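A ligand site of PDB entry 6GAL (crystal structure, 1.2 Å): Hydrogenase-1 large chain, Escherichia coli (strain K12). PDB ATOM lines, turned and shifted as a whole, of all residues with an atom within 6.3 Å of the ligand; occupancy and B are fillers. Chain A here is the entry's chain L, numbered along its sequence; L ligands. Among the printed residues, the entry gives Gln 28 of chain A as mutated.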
ATOM      1  N   GLN A  28       4.270  33.336  16.458  1.00  0.00           N
ATOM      2  CA  GLN A  28       2.843  33.503  16.647  1.00  0.00           C
ATOM      3  C   GLN A  28       2.374  32.615  17.774  1.00  0.00           C
ATOM      4  O   GLN A  28       2.774  31.438  17.820  1.00  0.00           O
ATOM      5  CB  GLN A  28       2.066  33.177  15.380  1.00  0.00           C
ATOM      6  CG  GLN A  28       0.583  33.561  15.425  1.00  0.00           C
ATOM      7  CD  GLN A  28      -0.288  32.777  16.407  1.00  0.00           C
ATOM      8  OE1 GLN A  28       0.006  31.591  16.641  1.00  0.00           O
ATOM      9  NE2 GLN A  28      -1.334  33.456  17.051  1.00  0.00           N
ATOM     10  N   ILE A  75      -8.089  30.215  12.354  1.00  0.00           N
ATOM     11  CA  ILE A  75      -7.020  29.495  13.004  1.00  0.00           C
ATOM     12  C   ILE A  75      -5.790  30.425  13.135  1.00  0.00           C
ATOM     13  O   ILE A  75      -5.043  30.344  14.119  1.00  0.00           O
ATOM     14  CB  ILE A  75      -6.701  28.160  12.321  1.00  0.00           C
ATOM     15  CG1 ILE A  75      -7.842  27.190  12.594  1.00  0.00           C
ATOM     16  CG2 ILE A  75      -5.373  27.578  12.795  1.00  0.00           C
ATOM     17  CD1 ILE A  75      -7.792  25.931  11.757  1.00  0.00           C
ATOM     18  N   CYS A  76      -5.518  31.206  12.089  1.00  0.00           N
ATOM     19  CA  CYS A  76      -4.316  32.003  12.066  1.00  0.00           C
ATOM     20  C   CYS A  76      -4.419  33.189  11.150  1.00  0.00           C
ATOM     21  O   CYS A  76      -4.748  33.045   9.989  1.00  0.00           O
ATOM     22  CB  CYS A  76      -3.165  31.118  11.625  1.00  0.00           C
ATOM     23  SG  CYS A  76      -1.550  31.929  11.834  1.00  0.00           S
ATOM     24  N   GLY A  77      -4.023  34.323  11.709  1.00  0.00           N
ATOM     25  CA  GLY A  77      -3.977  35.615  10.976  1.00  0.00           C
ATOM     26  C   GLY A  77      -2.632  35.913  10.361  1.00  0.00           C
ATOM     27  O   GLY A  77      -2.519  36.888   9.623  1.00  0.00           O
ATOM     28  N   VAL A  78      -1.626  35.082  10.638  1.00  0.00           N
ATOM     29  CA  VAL A  78      -0.263  35.213  10.052  1.00  0.00           C
ATOM     30  C   VAL A  78      -0.263  34.427   8.749  1.00  0.00           C
ATOM     31  O   VAL A  78      -0.060  35.002   7.667  1.00  0.00           O
ATOM     32  CB  VAL A  78       0.811  34.800  11.035  1.00  0.00           C
ATOM     33  CG1 VAL A  78       2.167  35.100  10.407  1.00  0.00           C
ATOM     34  CG2 VAL A  78       0.683  35.565  12.333  1.00  0.00           C
ATOM     35  N   CYS A  79      -0.570  33.138   8.807  1.00  0.00           N
ATOM     36  CA  CYS A  79      -0.774  32.351   7.592  1.00  0.00           C
ATOM     37  C   CYS A  79      -2.219  32.508   7.094  1.00  0.00           C
ATOM     38  O   CYS A  79      -2.914  31.580   6.798  1.00  0.00           O
ATOM     39  CB  CYS A  79      -0.355  30.930   7.762  1.00  0.00           C
ATOM     40  SG  CYS A  79      -1.165  29.951   9.062  1.00  0.00           S
ATOM     41  N   THR A  80      -2.663  33.753   7.056  1.00  0.00           N
ATOM     42  CA  THR A  80      -4.032  34.076   6.739  1.00  0.00           C
ATOM     43  C   THR A  80      -4.381  33.719   5.285  1.00  0.00           C
ATOM     44  O   THR A  80      -3.700  34.091   4.316  1.00  0.00           O
ATOM     45  CB  THR A  80      -4.346  35.545   7.005  1.00  0.00           C
ATOM     46  OG1 THR A  80      -5.734  35.798   6.778  1.00  0.00           O
ATOM     47  CG2 THR A  80      -3.547  36.515   6.103  1.00  0.00           C
ATOM     48  N   VAL A  82      -4.563  30.462   4.235  1.00  0.00           N
ATOM     49  CA  VAL A  82      -4.243  29.104   3.884  1.00  0.00           C
ATOM     50  C   VAL A  82      -5.279  28.110   4.385  1.00  0.00           C
ATOM     51  O   VAL A  82      -5.569  27.116   3.725  1.00  0.00           O
ATOM     52  CB  VAL A  82      -2.803  28.706   4.314  1.00  0.00           C
ATOM     53  CG1 VAL A  82      -2.676  28.489   5.801  1.00  0.00           C
ATOM     54  CG2 VAL A  82      -2.386  27.529   3.440  1.00  0.00           C
ATOM     55  N   HIS A  83      -5.848  28.365   5.575  1.00  0.00           N
ATOM     56  CA  HIS A  83      -6.860  27.468   6.104  1.00  0.00           C
ATOM     57  C   HIS A  83      -8.167  27.617   5.344  1.00  0.00           C
ATOM     58  O   HIS A  83      -8.915  26.644   5.205  1.00  0.00           O
ATOM     59  CB  HIS A  83      -7.078  27.734   7.575  1.00  0.00           C
ATOM     60  CG  HIS A  83      -5.949  27.293   8.420  1.00  0.00           C
ATOM     61  ND1 HIS A  83      -5.666  25.953   8.620  1.00  0.00           N
ATOM     62  CD2 HIS A  83      -4.961  27.995   9.036  1.00  0.00           C
ATOM     63  CE1 HIS A  83      -4.593  25.883   9.392  1.00  0.00           C
ATOM     64  NE2 HIS A  83      -4.122  27.099   9.628  1.00  0.00           N
ATOM     65  N   LEU A 114       0.577  34.975  -0.177  1.00  0.00           N
ATOM     66  CA  LEU A 114       0.830  34.693   1.204  1.00  0.00           C
ATOM     67  C   LEU A 114       2.243  34.155   1.436  1.00  0.00           C
ATOM     68  O   LEU A 114       2.913  34.602   2.389  1.00  0.00           O
ATOM     69  CB  LEU A 114      -0.207  33.707   1.748  1.00  0.00           C
ATOM     70  CG  LEU A 114       0.053  33.250   3.214  1.00  0.00           C
ATOM     71  CD1 LEU A 114      -0.105  34.427   4.144  1.00  0.00           C
ATOM     72  CD2 LEU A 114      -0.851  32.087   3.588  1.00  0.00           C
ATOM     73  N   ASP A 118       4.476  36.194   4.028  1.00  0.00           N
ATOM     74  CA  ASP A 118       4.743  35.515   5.285  1.00  0.00           C
ATOM     75  C   ASP A 118       6.238  35.204   5.400  1.00  0.00           C
ATOM     76  O   ASP A 118       6.857  35.404   6.475  1.00  0.00           O
ATOM     77  CB  ASP A 118       3.896  34.217   5.350  1.00  0.00           C
ATOM     78  CG  ASP A 118       3.550  33.711   6.723  1.00  0.00           C
ATOM     79  OD1 ASP A 118       4.319  34.005   7.636  1.00  0.00           O
ATOM     80  OD2 ASP A 118       2.607  32.905   6.809  1.00  0.00           O
ATOM     81  N   ALA A 507       1.211  25.279   3.267  1.00  0.00           N
ATOM     82  CA  ALA A 507       1.276  26.573   3.883  1.00  0.00           C
ATOM     83  C   ALA A 507       2.742  27.041   3.979  1.00  0.00           C
ATOM     84  O   ALA A 507       3.648  26.253   3.838  1.00  0.00           O
ATOM     85  CB  ALA A 507       0.645  26.551   5.257  1.00  0.00           C
ATOM     86  N   PRO A 508       2.958  28.323   4.261  1.00  0.00           N
ATOM     87  CA  PRO A 508       4.355  28.743   4.427  1.00  0.00           C
ATOM     88  C   PRO A 508       5.192  27.873   5.366  1.00  0.00           C
ATOM     89  O   PRO A 508       6.366  27.619   5.074  1.00  0.00           O
ATOM     90  CB  PRO A 508       4.236  30.176   4.936  1.00  0.00           C
ATOM     91  CG  PRO A 508       2.959  30.666   4.258  1.00  0.00           C
ATOM     92  CD  PRO A 508       2.038  29.460   4.298  1.00  0.00           C
ATOM     93  N   ARG A 509       4.576  27.357   6.425  1.00  0.00           N
ATOM     94  CA  ARG A 509       5.299  26.546   7.411  1.00  0.00           C
ATOM     95  C   ARG A 509       5.305  25.033   7.132  1.00  0.00           C
ATOM     96  O   ARG A 509       6.012  24.316   7.831  1.00  0.00           O
ATOM     97  CB  ARG A 509       4.732  26.833   8.792  1.00  0.00           C
ATOM     98  CG  ARG A 509       5.068  28.270   9.190  1.00  0.00           C
ATOM     99  CD  ARG A 509       4.147  28.802  10.246  1.00  0.00           C
ATOM    100  NE  ARG A 509       4.398  30.218  10.503  1.00  0.00           N
ATOM    101  CZ  ARG A 509       3.948  31.222   9.741  1.00  0.00           C
ATOM    102  NH1 ARG A 509       3.159  31.008   8.703  1.00  0.00           N
ATOM    103  NH2 ARG A 509       4.276  32.466  10.035  1.00  0.00           N
ATOM    104  N   GLY A 510       4.569  24.563   6.104  1.00  0.00           N
ATOM    105  CA  GLY A 510       4.602  23.158   5.719  1.00  0.00           C
ATOM    106  C   GLY A 510       3.260  22.573   5.367  1.00  0.00           C
ATOM    107  O   GLY A 510       2.300  23.286   5.083  1.00  0.00           O
ATOM    108  N   ALA A 511       3.216  21.266   5.407  1.00  0.00           N
ATOM    109  CA  ALA A 511       2.099  20.461   4.925  1.00  0.00           C
ATOM    110  C   ALA A 511       0.841  20.649   5.791  1.00  0.00           C
ATOM    111  O   ALA A 511       0.878  20.400   6.993  1.00  0.00           O
ATOM    112  CB  ALA A 511       2.515  18.990   4.932  1.00  0.00           C
ATOM    113  N   LEU A 512      -0.263  21.064   5.157  1.00  0.00           N
ATOM    114  CA  LEU A 512      -1.530  21.357   5.816  1.00  0.00           C
ATOM    115  C   LEU A 512      -2.607  20.439   5.234  1.00  0.00           C
ATOM    116  O   LEU A 512      -2.767  20.355   4.013  1.00  0.00           O
ATOM    117  CB  LEU A 512      -1.927  22.814   5.543  1.00  0.00           C
ATOM    118  CG  LEU A 512      -3.305  23.240   6.017  1.00  0.00           C
ATOM    119  CD1 LEU A 512      -3.443  23.090   7.535  1.00  0.00           C
ATOM    120  CD2 LEU A 512      -3.578  24.684   5.625  1.00  0.00           C
ATOM    121  N   VAL A 530      -1.867  20.577  11.070  1.00  0.00           N
ATOM    122  CA  VAL A 530      -1.304  21.811  10.555  1.00  0.00           C
ATOM    123  C   VAL A 530       0.211  21.729  10.622  1.00  0.00           C
ATOM    124  O   VAL A 530       0.758  20.965  11.396  1.00  0.00           O
ATOM    125  CB  VAL A 530      -1.938  22.954  11.377  1.00  0.00           C
ATOM    126  CG1 VAL A 530      -1.563  24.318  10.888  1.00  0.00           C
ATOM    127  CG2 VAL A 530      -3.465  22.817  11.401  1.00  0.00           C
ATOM    128  N   PRO A 531       0.957  22.499   9.806  1.00  0.00           N
ATOM    129  CA  PRO A 531       2.412  22.268   9.781  1.00  0.00           C
ATOM    130  C   PRO A 531       3.107  22.377  11.146  1.00  0.00           C
ATOM    131  O   PRO A 531       3.943  21.520  11.444  1.00  0.00           O
ATOM    132  CB  PRO A 531       2.941  23.293   8.780  1.00  0.00           C
ATOM    133  CG  PRO A 531       1.766  24.046   8.261  1.00  0.00           C
ATOM    134  CD  PRO A 531       0.529  23.313   8.649  1.00  0.00           C
ATOM    135  N   THR A 532       2.800  23.406  11.939  1.00  0.00           N
ATOM    136  CA  THR A 532       3.469  23.497  13.215  1.00  0.00           C
ATOM    137  C   THR A 532       2.988  22.355  14.144  1.00  0.00           C
ATOM    138  O   THR A 532       3.728  22.029  15.088  1.00  0.00           O
ATOM    139  CB  THR A 532       3.349  24.915  13.785  1.00  0.00           C
ATOM    140  OG1 THR A 532       3.928  25.865  12.883  1.00  0.00           O
ATOM    141  CG2 THR A 532       4.056  25.026  15.086  1.00  0.00           C
ATOM    142  N   THR A 533       1.813  21.762  13.924  1.00  0.00           N
ATOM    143  CA  THR A 533       1.462  20.543  14.681  1.00  0.00           C
ATOM    144  C   THR A 533       2.535  19.474  14.464  1.00  0.00           C
ATOM    145  O   THR A 533       2.991  18.841  15.397  1.00  0.00           O
ATOM    146  CB  THR A 533       0.081  19.972  14.267  1.00  0.00           C
ATOM    147  OG1 THR A 533      -0.869  21.027  14.099  1.00  0.00           O
ATOM    148  CG2 THR A 533      -0.399  18.974  15.301  1.00  0.00           C
ATOM    149  N   ASP A 574       9.816  29.091  11.792  1.00  0.00           N
ATOM    150  CA  ASP A 574       8.685  30.033  11.812  1.00  0.00           C
ATOM    151  C   ASP A 574       7.491  29.438  12.576  1.00  0.00           C
ATOM    152  O   ASP A 574       6.440  29.154  12.015  1.00  0.00           O
ATOM    153  CB  ASP A 574       8.308  30.441  10.338  1.00  0.00           C
ATOM    154  CG  ASP A 574       7.367  31.652  10.242  1.00  0.00           C
ATOM    155  OD1 ASP A 574       6.872  32.111  11.268  1.00  0.00           O
ATOM    156  OD2 ASP A 574       7.114  32.179   9.114  1.00  0.00           O
ATOM    157  N   PRO A 575       7.654  29.211  13.884  1.00  0.00           N
ATOM    158  CA  PRO A 575       6.562  28.575  14.624  1.00  0.00           C
ATOM    159  C   PRO A 575       5.259  29.372  14.642  1.00  0.00           C
ATOM    160  O   PRO A 575       5.259  30.572  14.908  1.00  0.00           O
ATOM    161  CB  PRO A 575       7.127  28.453  16.055  1.00  0.00           C
ATOM    162  CG  PRO A 575       8.642  28.511  15.876  1.00  0.00           C
ATOM    163  CD  PRO A 575       8.828  29.450  14.728  1.00  0.00           C
ATOM    164  N   CYS A 576       4.159  28.668  14.423  1.00  0.00           N
ATOM    165  CA  CYS A 576       2.845  29.269  14.466  1.00  0.00           C
ATOM    166  C   CYS A 576       2.018  28.409  15.445  1.00  0.00           C
ATOM    167  O   CYS A 576       1.512  27.342  15.092  1.00  0.00           O
ATOM    168  CB  CYS A 576       2.215  29.275  13.068  1.00  0.00           C
ATOM    169  SG  CYS A 576       0.676  30.218  13.021  1.00  0.00           S
ATOM    170  N   LEU A 577       1.907  28.876  16.682  1.00  0.00           N
ATOM    171  CA  LEU A 577       1.368  28.055  17.702  1.00  0.00           C
ATOM    172  C   LEU A 577      -0.163  28.023  17.684  1.00  0.00           C
ATOM    173  O   LEU A 577      -0.732  26.993  18.055  1.00  0.00           O
ATOM    174  CB  LEU A 577       1.897  28.468  19.075  1.00  0.00           C
ATOM    175  CG  LEU A 577       3.261  27.860  19.383  1.00  0.00           C
ATOM    176  CD1 LEU A 577       3.155  26.383  19.762  1.00  0.00           C
ATOM    177  CD2 LEU A 577       4.294  28.065  18.313  1.00  0.00           C
ATOM    178  N   ALA A 578      -0.803  29.071  17.216  1.00  0.00           N
ATOM    179  CA  ALA A 578      -2.259  29.036  17.028  1.00  0.00           C
ATOM    180  C   ALA A 578      -2.626  28.038  15.938  1.00  0.00           C
ATOM    181  O   ALA A 578      -3.582  27.270  16.056  1.00  0.00           O
ATOM    182  CB  ALA A 578      -2.801  30.425  16.722  1.00  0.00           C
ATOM    183  N   CYS A 579      -1.822  28.027  14.892  1.00  0.00           N
ATOM    184  CA  CYS A 579      -1.939  26.974  13.886  1.00  0.00           C
ATOM    185  C   CYS A 579      -1.796  25.598  14.470  1.00  0.00           C
ATOM    186  O   CYS A 579      -2.571  24.698  14.148  1.00  0.00           O
ATOM    187  CB  CYS A 579      -0.911  27.130  12.753  1.00  0.00           C
ATOM    188  SG  CYS A 579      -1.454  28.156  11.400  1.00  0.00           S
ATOM    189  N   SER A 580      -0.781  25.427  15.327  1.00  0.00           N
ATOM    190  CA  SER A 580      -0.443  24.060  15.767  1.00  0.00           C
ATOM    191  C   SER A 580      -1.538  23.433  16.601  1.00  0.00           C
ATOM    192  O   SER A 580      -1.694  22.201  16.562  1.00  0.00           O
ATOM    193  CB  SER A 580       0.864  24.085  16.557  1.00  0.00           C
ATOM    194  OG  SER A 580       0.698  24.604  17.864  1.00  0.00           O
HETATM  195 FE1  LIG L   1      -0.015  28.075   9.632  1.00  0.00          FE
HETATM  196 NI1  LIG L   1      -0.260  30.211  11.158  1.00  0.00          NI
HETATM  197  C1  LIG L   1       1.090  26.904  10.529  1.00  0.00           C
HETATM  198  N1  LIG L   1       1.775  26.128  11.070  1.00  0.00           N
HETATM  199  C2  LIG L   1       1.296  28.317   8.289  1.00  0.00           C
HETATM  200  N2  LIG L   1       2.108  28.400   7.448  1.00  0.00           N
HETATM  201  C3  LIG L   1      -0.804  26.846   8.651  1.00  0.00           C
HETATM  202  O1  LIG L   1      -1.305  26.070   7.987  1.00  0.00           O
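A nickel atom (NI1) of the ligand is bound by the side-chain sulfur of Cys 576, at 2.1 Å.
NI1 of the ligand is bound by SG of Cys 76 (2.3 Å).
FE1 of the ligand is bound by SG of Cys 79 (2.3 Å).
An iron atom (FE1) of the ligand is bound by the side-chain sulfur (SG) of Cys 579.
A nitrogen (N1) of the ligand is in hydrogen-bond range of the backbone NH (N) of Thr 532, 3.0 Å away.
The side-chain hydroxyl of Thr 532 lies within hydrogen-bond range of a nitrogen (N1) of the ligand (2.8 Å).
N2 of the ligand lies within hydrogen-bond range of N of Arg 509 (2.9 Å).
NH1 of Arg 509 sits at hydrogen-bond distance from N2 of the ligand.
O1 of the ligand lies within hydrogen-bond range of NE2 of His 83.
N of Cys 576 lies within hydrogen-bond range of OG1 of Thr 532 (3.2 Å).
The backbone NH (N) of Val 78 sits close to the side-chain sulfur (SG) of Cys 76 (3.4 Å).
The side-chain sulfur (SG) of Cys 579 lies close to a ring nitrogen (NE2) of His 83 (3.4 Å).
The guanidinium group (NH1) of Arg 509 lies within salt-bridge range of the side-chain carboxylate (OD2) of Asp 118, at 2.7 Å.
The side-chain carboxylate (OD1) of Asp 574 is in salt-bridge range of the guanidinium group (NH2) of Arg 509 (2.9 Å).
The backbone carbonyl oxygen of Val 530 lies close to the side-chain hydroxyl of Thr 533, at 3.2 Å.
The backbone nitrogen (N) of Pro 508 sits close to a nitrogen (N2) of the ligand (3.3 Å).
Merely in contact with the ligand: Val 82, Ala 507, Leu 512, Val 530 and Pro 531.
The nearest printed residue that does not touch the ligand is Asp 118 (4.6 Å).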
